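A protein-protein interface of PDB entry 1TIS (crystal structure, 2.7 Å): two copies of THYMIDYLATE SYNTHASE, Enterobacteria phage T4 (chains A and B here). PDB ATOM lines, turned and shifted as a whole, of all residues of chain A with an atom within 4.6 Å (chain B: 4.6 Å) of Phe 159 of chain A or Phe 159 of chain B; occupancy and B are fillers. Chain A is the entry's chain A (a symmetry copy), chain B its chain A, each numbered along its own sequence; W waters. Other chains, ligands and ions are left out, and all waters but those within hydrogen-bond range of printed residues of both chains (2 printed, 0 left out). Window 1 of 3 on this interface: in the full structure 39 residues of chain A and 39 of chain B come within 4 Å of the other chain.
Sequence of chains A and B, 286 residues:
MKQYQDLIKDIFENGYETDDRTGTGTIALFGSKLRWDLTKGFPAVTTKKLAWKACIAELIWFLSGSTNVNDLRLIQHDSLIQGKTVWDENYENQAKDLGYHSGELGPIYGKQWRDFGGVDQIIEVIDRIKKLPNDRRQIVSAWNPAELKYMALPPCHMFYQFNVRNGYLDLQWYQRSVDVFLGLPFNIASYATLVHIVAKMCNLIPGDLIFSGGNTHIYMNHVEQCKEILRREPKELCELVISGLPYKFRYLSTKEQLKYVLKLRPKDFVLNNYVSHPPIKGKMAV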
ATOM      1  N   ILE A 139     -31.122   0.279  -4.374  1.00  0.00           N
ATOM      2  CA  ILE A 139     -30.938  -1.052  -3.748  1.00  0.00           C
ATOM      3  C   ILE A 139     -32.116  -2.031  -3.890  1.00  0.00           C
ATOM      4  O   ILE A 139     -33.221  -1.488  -3.784  1.00  0.00           O
ATOM      5  CB  ILE A 139     -30.661  -0.819  -2.234  1.00  0.00           C
ATOM      6  CG1 ILE A 139     -29.553   0.174  -2.059  1.00  0.00           C
ATOM      7  CG2 ILE A 139     -30.288  -2.109  -1.552  1.00  0.00           C
ATOM      8  CD1 ILE A 139     -29.111   0.269  -0.605  1.00  0.00           C
ATOM      9  N   VAL A 140     -32.093  -3.359  -4.130  1.00  0.00           N
ATOM     10  CA  VAL A 140     -33.336  -4.112  -3.988  1.00  0.00           C
ATOM     11  C   VAL A 140     -33.064  -5.350  -3.140  1.00  0.00           C
ATOM     12  O   VAL A 140     -32.340  -6.282  -3.442  1.00  0.00           O
ATOM     13  CB  VAL A 140     -34.059  -4.499  -5.396  1.00  0.00           C
ATOM     14  CG1 VAL A 140     -33.519  -3.628  -6.486  1.00  0.00           C
ATOM     15  CG2 VAL A 140     -33.921  -5.943  -5.806  1.00  0.00           C
ATOM     16  N   SER A 141     -33.568  -5.283  -1.930  1.00  0.00           N
ATOM     17  CA  SER A 141     -33.424  -6.315  -0.938  1.00  0.00           C
ATOM     18  C   SER A 141     -34.431  -7.368  -1.297  1.00  0.00           C
ATOM     19  O   SER A 141     -35.539  -7.015  -1.722  1.00  0.00           O
ATOM     20  CB  SER A 141     -33.739  -5.731   0.417  1.00  0.00           C
ATOM     21  OG  SER A 141     -33.772  -6.691   1.468  1.00  0.00           O
ATOM     22  N   TRP A 143     -34.441 -10.281   0.958  1.00  0.00           N
ATOM     23  CA  TRP A 143     -34.666 -10.919   2.234  1.00  0.00           C
ATOM     24  C   TRP A 143     -35.731 -10.083   2.908  1.00  0.00           C
ATOM     25  O   TRP A 143     -35.595  -8.880   3.136  1.00  0.00           O
ATOM     26  CB  TRP A 143     -33.380 -10.906   2.992  1.00  0.00           C
ATOM     27  CG  TRP A 143     -33.348 -11.587   4.341  1.00  0.00           C
ATOM     28  CD1 TRP A 143     -33.480 -10.857   5.502  1.00  0.00           C
ATOM     29  CD2 TRP A 143     -33.026 -12.903   4.564  1.00  0.00           C
ATOM     30  NE1 TRP A 143     -33.209 -11.711   6.453  1.00  0.00           N
ATOM     31  CE2 TRP A 143     -32.935 -12.928   5.938  1.00  0.00           C
ATOM     32  CE3 TRP A 143     -32.766 -14.047   3.846  1.00  0.00           C
ATOM     33  CZ2 TRP A 143     -32.585 -14.086   6.600  1.00  0.00           C
ATOM     34  CZ3 TRP A 143     -32.411 -15.200   4.517  1.00  0.00           C
ATOM     35  CH2 TRP A 143     -32.320 -15.224   5.885  1.00  0.00           C
ATOM     36  N   HIS A 157     -29.160 -15.287  -2.931  1.00  0.00           N
ATOM     37  CA  HIS A 157     -28.758 -13.959  -3.371  1.00  0.00           C
ATOM     38  C   HIS A 157     -29.853 -12.992  -2.888  1.00  0.00           C
ATOM     39  O   HIS A 157     -31.009 -13.033  -3.350  1.00  0.00           O
ATOM     40  CB  HIS A 157     -28.580 -13.911  -4.912  1.00  0.00           C
ATOM     41  CG  HIS A 157     -29.455 -14.742  -5.849  1.00  0.00           C
ATOM     42  ND1 HIS A 157     -29.411 -16.046  -6.008  1.00  0.00           N
ATOM     43  CD2 HIS A 157     -30.402 -14.263  -6.736  1.00  0.00           C
ATOM     44  CE1 HIS A 157     -30.284 -16.365  -6.944  1.00  0.00           C
ATOM     45  NE2 HIS A 157     -30.880 -15.302  -7.381  1.00  0.00           N
ATOM     46  N   MET A 158     -29.515 -12.120  -1.929  1.00  0.00           N
ATOM     47  CA  MET A 158     -30.523 -11.313  -1.266  1.00  0.00           C
ATOM     48  C   MET A 158     -30.523  -9.818  -1.399  1.00  0.00           C
ATOM     49  O   MET A 158     -31.503  -9.178  -1.038  1.00  0.00           O
ATOM     50  CB  MET A 158     -30.485 -11.616   0.192  1.00  0.00           C
ATOM     51  CG  MET A 158     -29.153 -11.248   0.817  1.00  0.00           C
ATOM     52  SD  MET A 158     -29.104 -12.015   2.455  1.00  0.00           S
ATOM     53  CE  MET A 158     -28.909 -13.590   1.681  1.00  0.00           C
ATOM     54  N   PHE A 159     -29.484  -9.239  -1.948  1.00  0.00           N
ATOM     55  CA  PHE A 159     -29.309  -7.815  -1.890  1.00  0.00           C
ATOM     56  C   PHE A 159     -28.614  -7.367  -3.139  1.00  0.00           C
ATOM     57  O   PHE A 159     -27.992  -8.241  -3.759  1.00  0.00           O
ATOM     58  CB  PHE A 159     -28.477  -7.619  -0.714  1.00  0.00           C
ATOM     59  CG  PHE A 159     -28.872  -6.458   0.107  1.00  0.00           C
ATOM     60  CD1 PHE A 159     -30.153  -6.413   0.628  1.00  0.00           C
ATOM     61  CD2 PHE A 159     -27.928  -5.496   0.346  1.00  0.00           C
ATOM     62  CE1 PHE A 159     -30.517  -5.359   1.428  1.00  0.00           C
ATOM     63  CE2 PHE A 159     -28.293  -4.441   1.147  1.00  0.00           C
ATOM     64  CZ  PHE A 159     -29.575  -4.378   1.680  1.00  0.00           C
ATOM     65  N   TYR A 160     -28.690  -6.075  -3.507  1.00  0.00           N
ATOM     66  CA  TYR A 160     -27.842  -5.484  -4.555  1.00  0.00           C
ATOM     67  C   TYR A 160     -28.005  -3.995  -4.667  1.00  0.00           C
ATOM     68  O   TYR A 160     -29.066  -3.440  -4.375  1.00  0.00           O
ATOM     69  CB  TYR A 160     -28.035  -6.063  -5.983  1.00  0.00           C
ATOM     70  CG  TYR A 160     -29.357  -6.260  -6.687  1.00  0.00           C
ATOM     71  CD1 TYR A 160     -29.906  -5.196  -7.375  1.00  0.00           C
ATOM     72  CD2 TYR A 160     -29.959  -7.514  -6.745  1.00  0.00           C
ATOM     73  CE1 TYR A 160     -31.041  -5.361  -8.131  1.00  0.00           C
ATOM     74  CE2 TYR A 160     -31.107  -7.687  -7.514  1.00  0.00           C
ATOM     75  CZ  TYR A 160     -31.635  -6.597  -8.195  1.00  0.00           C
ATOM     76  OH  TYR A 160     -32.809  -6.711  -8.921  1.00  0.00           O
ATOM     77  N   GLN A 172     -23.901  -4.808  -7.717  1.00  0.00           N
ATOM     78  CA  GLN A 172     -23.183  -5.634  -6.746  1.00  0.00           C
ATOM     79  C   GLN A 172     -24.142  -6.475  -5.894  1.00  0.00           C
ATOM     80  O   GLN A 172     -24.991  -5.943  -5.196  1.00  0.00           O
ATOM     81  CB  GLN A 172     -22.325  -4.724  -5.847  1.00  0.00           C
ATOM     82  CG  GLN A 172     -21.823  -5.481  -4.654  1.00  0.00           C
ATOM     83  CD  GLN A 172     -20.908  -4.661  -3.821  1.00  0.00           C
ATOM     84  OE1 GLN A 172     -19.808  -5.126  -3.586  1.00  0.00           O
ATOM     85  NE2 GLN A 172     -21.214  -3.458  -3.378  1.00  0.00           N
ATOM     86  N   TRP A 173     -24.015  -7.770  -5.865  1.00  0.00           N
ATOM     87  CA  TRP A 173     -24.899  -8.611  -5.087  1.00  0.00           C
ATOM     88  C   TRP A 173     -24.214  -9.059  -3.834  1.00  0.00           C
ATOM     89  O   TRP A 173     -22.967  -9.044  -3.726  1.00  0.00           O
ATOM     90  CB  TRP A 173     -25.370  -9.887  -5.853  1.00  0.00           C
ATOM     91  CG  TRP A 173     -24.465 -10.471  -6.926  1.00  0.00           C
ATOM     92  CD1 TRP A 173     -23.838  -9.748  -7.934  1.00  0.00           C
ATOM     93  CD2 TRP A 173     -24.122 -11.769  -6.978  1.00  0.00           C
ATOM     94  NE1 TRP A 173     -23.082 -10.587  -8.606  1.00  0.00           N
ATOM     95  CE2 TRP A 173     -23.230 -11.799  -8.058  1.00  0.00           C
ATOM     96  CE3 TRP A 173     -24.462 -12.860  -6.238  1.00  0.00           C
ATOM     97  CZ2 TRP A 173     -22.617 -12.954  -8.452  1.00  0.00           C
ATOM     98  CZ3 TRP A 173     -23.846 -14.025  -6.630  1.00  0.00           C
ATOM     99  CH2 TRP A 173     -22.944 -14.070  -7.708  1.00  0.00           C
ATOM    100  N   TYR A 174     -25.041  -9.405  -2.864  1.00  0.00           N
ATOM    101  CA  TYR A 174     -24.488 -10.065  -1.685  1.00  0.00           C
ATOM    102  C   TYR A 174     -25.143 -11.450  -1.676  1.00  0.00           C
ATOM    103  O   TYR A 174     -26.347 -11.574  -1.935  1.00  0.00           O
ATOM    104  CB  TYR A 174     -24.831  -9.267  -0.454  1.00  0.00           C
ATOM    105  CG  TYR A 174     -24.221  -9.826   0.798  1.00  0.00           C
ATOM    106  CD1 TYR A 174     -24.746 -10.975   1.378  1.00  0.00           C
ATOM    107  CD2 TYR A 174     -23.154  -9.157   1.343  1.00  0.00           C
ATOM    108  CE1 TYR A 174     -24.187 -11.471   2.534  1.00  0.00           C
ATOM    109  CE2 TYR A 174     -22.600  -9.642   2.505  1.00  0.00           C
ATOM    110  CZ  TYR A 174     -23.127 -10.783   3.074  1.00  0.00           C
ATOM    111  OH  TYR A 174     -22.587 -11.229   4.235  1.00  0.00           O
ATOM    112  N   ILE B 139     -28.654 -13.606   9.666  1.00  0.00           N
ATOM    113  CA  ILE B 139     -28.616 -12.289   8.989  1.00  0.00           C
ATOM    114  C   ILE B 139     -29.489 -11.186   9.613  1.00  0.00           C
ATOM    115  O   ILE B 139     -30.579 -11.597  10.024  1.00  0.00           O
ATOM    116  CB  ILE B 139     -29.070 -12.511   7.516  1.00  0.00           C
ATOM    117  CG1 ILE B 139     -28.277 -13.619   6.893  1.00  0.00           C
ATOM    118  CG2 ILE B 139     -28.895 -11.255   6.705  1.00  0.00           C
ATOM    119  CD1 ILE B 139     -28.542 -13.725   5.397  1.00  0.00           C
ATOM    120  N   VAL B 140     -29.210  -9.877   9.783  1.00  0.00           N
ATOM    121  CA  VAL B 140     -30.292  -8.983  10.188  1.00  0.00           C
ATOM    122  C   VAL B 140     -30.286  -7.762   9.274  1.00  0.00           C
ATOM    123  O   VAL B 140     -29.403  -6.927   9.197  1.00  0.00           O
ATOM    124  CB  VAL B 140     -30.264  -8.554  11.760  1.00  0.00           C
ATOM    125  CG1 VAL B 140     -29.399  -9.510  12.518  1.00  0.00           C
ATOM    126  CG2 VAL B 140     -29.795  -7.147  12.026  1.00  0.00           C
ATOM    127  N   SER B 141     -31.280  -7.739   8.417  1.00  0.00           N
ATOM    128  CA  SER B 141     -31.475  -6.704   7.437  1.00  0.00           C
ATOM    129  C   SER B 141     -32.090  -5.552   8.178  1.00  0.00           C
ATOM    130  O   SER B 141     -32.926  -5.788   9.061  1.00  0.00           O
ATOM    131  CB  SER B 141     -32.424  -7.211   6.379  1.00  0.00           C
ATOM    132  OG  SER B 141     -32.812  -6.226   5.428  1.00  0.00           O
ATOM    133  N   TRP B 143     -32.770  -2.598   6.086  1.00  0.00           N
ATOM    134  CA  TRP B 143     -33.465  -1.905   5.026  1.00  0.00           C
ATOM    135  C   TRP B 143     -34.806  -2.595   4.918  1.00  0.00           C
ATOM    136  O   TRP B 143     -34.924  -3.800   4.686  1.00  0.00           O
ATOM    137  CB  TRP B 143     -32.661  -2.043   3.776  1.00  0.00           C
ATOM    138  CG  TRP B 143     -33.155  -1.335   2.535  1.00  0.00           C
ATOM    139  CD1 TRP B 143     -33.871  -2.014   1.575  1.00  0.00           C
ATOM    140  CD2 TRP B 143     -32.818  -0.059   2.157  1.00  0.00           C
ATOM    141  NE1 TRP B 143     -33.956  -1.171   0.579  1.00  0.00           N
ATOM    142  CE2 TRP B 143     -33.345  -0.007   0.887  1.00  0.00           C
ATOM    143  CE3 TRP B 143     -32.137   1.029   2.654  1.00  0.00           C
ATOM    144  CZ2 TRP B 143     -33.197   1.121   0.107  1.00  0.00           C
ATOM    145  CZ3 TRP B 143     -31.989   2.151   1.864  1.00  0.00           C
ATOM    146  CH2 TRP B 143     -32.514   2.201   0.599  1.00  0.00           C
ATOM    147  N   HIS B 157     -25.779   1.667   7.085  1.00  0.00           N
ATOM    148  CA  HIS B 157     -25.377   0.291   7.335  1.00  0.00           C
ATOM    149  C   HIS B 157     -26.675  -0.531   7.416  1.00  0.00           C
ATOM    150  O   HIS B 157     -27.492  -0.371   8.342  1.00  0.00           O
ATOM    151  CB  HIS B 157     -24.540   0.182   8.638  1.00  0.00           C
ATOM    152  CG  HIS B 157     -24.806   1.082   9.843  1.00  0.00           C
ATOM    153  ND1 HIS B 157     -24.547   2.367   9.931  1.00  0.00           N
ATOM    154  CD2 HIS B 157     -25.307   0.689  11.071  1.00  0.00           C
ATOM    155  CE1 HIS B 157     -24.870   2.758  11.149  1.00  0.00           C
ATOM    156  NE2 HIS B 157     -25.326   1.759  11.834  1.00  0.00           N
ATOM    157  N   MET B 158     -26.901  -1.411   6.430  1.00  0.00           N
ATOM    158  CA  MET B 158     -28.182  -2.079   6.307  1.00  0.00           C
ATOM    159  C   MET B 158     -28.293  -3.567   6.466  1.00  0.00           C
ATOM    160  O   MET B 158     -29.398  -4.081   6.595  1.00  0.00           O
ATOM    161  CB  MET B 158     -28.763  -1.744   4.977  1.00  0.00           C
ATOM    162  CG  MET B 158     -27.900  -2.244   3.835  1.00  0.00           C
ATOM    163  SD  MET B 158     -28.497  -1.444   2.325  1.00  0.00           S
ATOM    164  CE  MET B 158     -27.800   0.077   2.890  1.00  0.00           C
ATOM    165  N   PHE B 159     -27.193  -4.276   6.511  1.00  0.00           N
ATOM    166  CA  PHE B 159     -27.225  -5.708   6.419  1.00  0.00           C
ATOM    167  C   PHE B 159     -26.103  -6.266   7.241  1.00  0.00           C
ATOM    168  O   PHE B 159     -25.176  -5.485   7.496  1.00  0.00           O
ATOM    169  CB  PHE B 159     -27.031  -5.966   5.002  1.00  0.00           C
ATOM    170  CG  PHE B 159     -27.879  -7.052   4.474  1.00  0.00           C
ATOM    171  CD1 PHE B 159     -29.254  -6.937   4.578  1.00  0.00           C
ATOM    172  CD2 PHE B 159     -27.256  -8.109   3.866  1.00  0.00           C
ATOM    173  CE1 PHE B 159     -30.054  -7.921   4.052  1.00  0.00           C
ATOM    174  CE2 PHE B 159     -28.058  -9.093   3.339  1.00  0.00           C
ATOM    175  CZ  PHE B 159     -29.441  -8.996   3.433  1.00  0.00           C
ATOM    176  N   TYR B 160     -26.155  -7.550   7.639  1.00  0.00           N
ATOM    177  CA  TYR B 160     -25.003  -8.262   8.215  1.00  0.00           C
ATOM    178  C   TYR B 160     -25.267  -9.725   8.428  1.00  0.00           C
ATOM    179  O   TYR B 160     -26.403 -10.147   8.653  1.00  0.00           O
ATOM    180  CB  TYR B 160     -24.473  -7.703   9.565  1.00  0.00           C
ATOM    181  CG  TYR B 160     -25.312  -7.376  10.777  1.00  0.00           C
ATOM    182  CD1 TYR B 160     -25.615  -8.388  11.666  1.00  0.00           C
ATOM    183  CD2 TYR B 160     -25.678  -6.063  11.063  1.00  0.00           C
ATOM    184  CE1 TYR B 160     -26.269  -8.116  12.843  1.00  0.00           C
ATOM    185  CE2 TYR B 160     -26.336  -5.782  12.257  1.00  0.00           C
ATOM    186  CZ  TYR B 160     -26.626  -6.822  13.131  1.00  0.00           C
ATOM    187  OH  TYR B 160     -27.334  -6.594  14.300  1.00  0.00           O
ATOM    188  N   GLN B 172     -20.173  -9.468   9.312  1.00  0.00           N
ATOM    189  CA  GLN B 172     -19.872  -8.703   8.101  1.00  0.00           C
ATOM    190  C   GLN B 172     -21.007  -7.735   7.742  1.00  0.00           C
ATOM    191  O   GLN B 172     -22.132  -8.148   7.509  1.00  0.00           O
ATOM    192  CB  GLN B 172     -19.613  -9.680   6.939  1.00  0.00           C
ATOM    193  CG  GLN B 172     -19.612  -8.953   5.628  1.00  0.00           C
ATOM    194  CD  GLN B 172     -19.262  -9.850   4.497  1.00  0.00           C
ATOM    195  OE1 GLN B 172     -18.336  -9.507   3.785  1.00  0.00           O
ATOM    196  NE2 GLN B 172     -19.868 -10.997   4.268  1.00  0.00           N
ATOM    197  N   TRP B 173     -20.760  -6.463   7.625  1.00  0.00           N
ATOM    198  CA  TRP B 173     -21.795  -5.506   7.299  1.00  0.00           C
ATOM    199  C   TRP B 173     -21.693  -5.106   5.861  1.00  0.00           C
ATOM    200  O   TRP B 173     -20.635  -5.259   5.210  1.00  0.00           O
ATOM    201  CB  TRP B 173     -21.728  -4.205   8.160  1.00  0.00           C
ATOM    202  CG  TRP B 173     -20.380  -3.758   8.703  1.00  0.00           C
ATOM    203  CD1 TRP B 173     -19.457  -4.574   9.345  1.00  0.00           C
ATOM    204  CD2 TRP B 173     -19.905  -2.509   8.562  1.00  0.00           C
ATOM    205  NE1 TRP B 173     -18.391  -3.845   9.588  1.00  0.00           N
ATOM    206  CE2 TRP B 173     -18.628  -2.610   9.132  1.00  0.00           C
ATOM    207  CE3 TRP B 173     -20.411  -1.367   8.021  1.00  0.00           C
ATOM    208  CZ2 TRP B 173     -17.777  -1.544   9.180  1.00  0.00           C
ATOM    209  CZ3 TRP B 173     -19.557  -0.290   8.067  1.00  0.00           C
ATOM    210  CH2 TRP B 173     -18.270  -0.378   8.630  1.00  0.00           C
ATOM    211  N   TYR B 174     -22.820  -4.641   5.351  1.00  0.00           N
ATOM    212  CA  TYR B 174     -22.777  -4.018   4.031  1.00  0.00           C
ATOM    213  C   TYR B 174     -23.205  -2.567   4.278  1.00  0.00           C
ATOM    214  O   TYR B 174     -24.145  -2.314   5.042  1.00  0.00           O
ATOM    215  CB  TYR B 174     -23.720  -4.738   3.103  1.00  0.00           C
ATOM    216  CG  TYR B 174     -23.671  -4.218   1.697  1.00  0.00           C
ATOM    217  CD1 TYR B 174     -24.264  -3.003   1.379  1.00  0.00           C
ATOM    218  CD2 TYR B 174     -23.042  -4.990   0.752  1.00  0.00           C
ATOM    219  CE1 TYR B 174     -24.225  -2.543   0.083  1.00  0.00           C
ATOM    220  CE2 TYR B 174     -23.011  -4.541  -0.548  1.00  0.00           C
ATOM    221  CZ  TYR B 174     -23.602  -3.332  -0.853  1.00  0.00           C
ATOM    222  OH  TYR B 174     -23.588  -2.920  -2.145  1.00  0.00           O
HETATM  223  O   HOH W   1     -33.378 -11.431   9.285  1.00  0.00           O
HETATM  224  O   HOH W   2     -35.397  -1.354  -1.873  1.00  0.00           O
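Printed residues of chain A that touch a printed residue of chain B: Ile 139, Ser 141, Trp 143, Met 158, Phe 159, Gln 172 and Tyr 174.
Hydrophobic or aromatic side chains of chain A within 4 Å of the printed part of chain B: Ile 139, Trp 143, Met 158, Phe 159 and Tyr 174.
Along chain B the printed residues that touch a printed residue of chain A span positions 139 to 174.
Among the printed residues, 11 pairs touch across the chains.
Among the printed residues, no Asp or Glu carboxylate lies within 4 Å of a Lys or Arg side-chain nitrogen of the other chain.
The backbone NH (N) of Met 158 of chain A sits at hydrogen-bond distance from the backbone carbonyl oxygen (O) of Tyr 174 of chain A, at 3.2 Å.
The side-chain hydroxyl (OG) of Ser 141 of chain A is in hydrogen-bond range of the backbone carbonyl oxygen (O) of Trp 143 of chain A, 3.3 Å away.
OG of Ser 141 of chain B lies within hydrogen-bond range of O of Trp 143 of chain B (3.3 Å).
The backbone carbonyl oxygen (O) of Phe 159 of chain A sits at hydrogen-bond distance from the backbone NH (N) of Tyr 174 of chain A (3.3 Å).
The backbone NH (N) of Tyr 174 of chain B lies within hydrogen-bond range of the backbone carbonyl oxygen (O) of Phe 159 of chain B, at 3.3 Å.
The backbone carbonyl oxygen (O) of Tyr 174 of chain B is in hydrogen-bond range of the backbone NH (N) of Met 158 of chain B.
Ile 139 of chain A touches Trp 143 of chain B, and with the chains exchanged Trp 143 of chain A touches Ile 139 of chain B.
Ser 141 of chain A touches Trp 143 of chain B, and with the chains exchanged Trp 143 of chain A touches Ser 141 of chain B.
Phe 159 of chain B touches its own counterpart, Phe 159 of chain A.
Gln 172 of chain A touches Tyr 174 of chain B, and with the chains exchanged Tyr 174 of chain A touches Gln 172 of chain B.
11 positions are printed for both chains.
Ile 139 of chain A touches Trp 143 of chain B.
Met 158 of chain B touches Ile 139 of chain A (SD to CD1, 3.4 Å).
CB of Ser 141 of chain A touches CD1 of Trp 143 of chain B, at 3.9 Å.
CZ2 of Trp 143 of chain A touches CB of Ile 139 of chain B, 3.96 Å away.
Trp 143 of chain A touches Ser 141 of chain B (CD1 to CB, 3.9 Å).
Met 158 of chain A touches Ile 139 of chain B.
Met 158 of chain A touches Phe 159 of chain B (SD to CZ, 3.2 Å).
SD of Met 158 of chain B touches CZ of Phe 159 of chain A (3.2 Å).
CE1 of Phe 159 of chain B touches CE1 of Phe 159 of chain A, 3.7 Å away.
Printed residues of chain B within 4 Å of Ser 141 of chain A: Trp 143.
Of the printed residues of chain A, Trp 143 of chain B touches Ile 139 (3.96 Å) and Ser 141 (3.9 Å).
Of chain A, only Met 158 (3.2 Å) and Phe 159 (3.7 Å) come within 4 Å of Phe 159 of chain B.
The nearest residue of chain A that does not touch Phe 159 of chain B is Tyr 174 of chain A (4.3 Å).
Water W1 lies within hydrogen-bond range of NE1 of Trp 143 of chain A and O of Ile 139 of chain B.
Water W2 bridges NE1 of Trp 143 of chain B (2.8 Å) and O of Ile 139 of chain A (2.9 Å).
The side-chain amide nitrogen of Gln 172 of chain B lies within hydrogen-bond range of the side-chain hydroxyl of Tyr 174 of chain A (2.7 Å).
The side-chain amide nitrogen (NE2) of Gln 172 of chain A is in hydrogen-bond range of the side-chain hydroxyl (OH) of Tyr 174 of chain B, at 2.7 Å.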
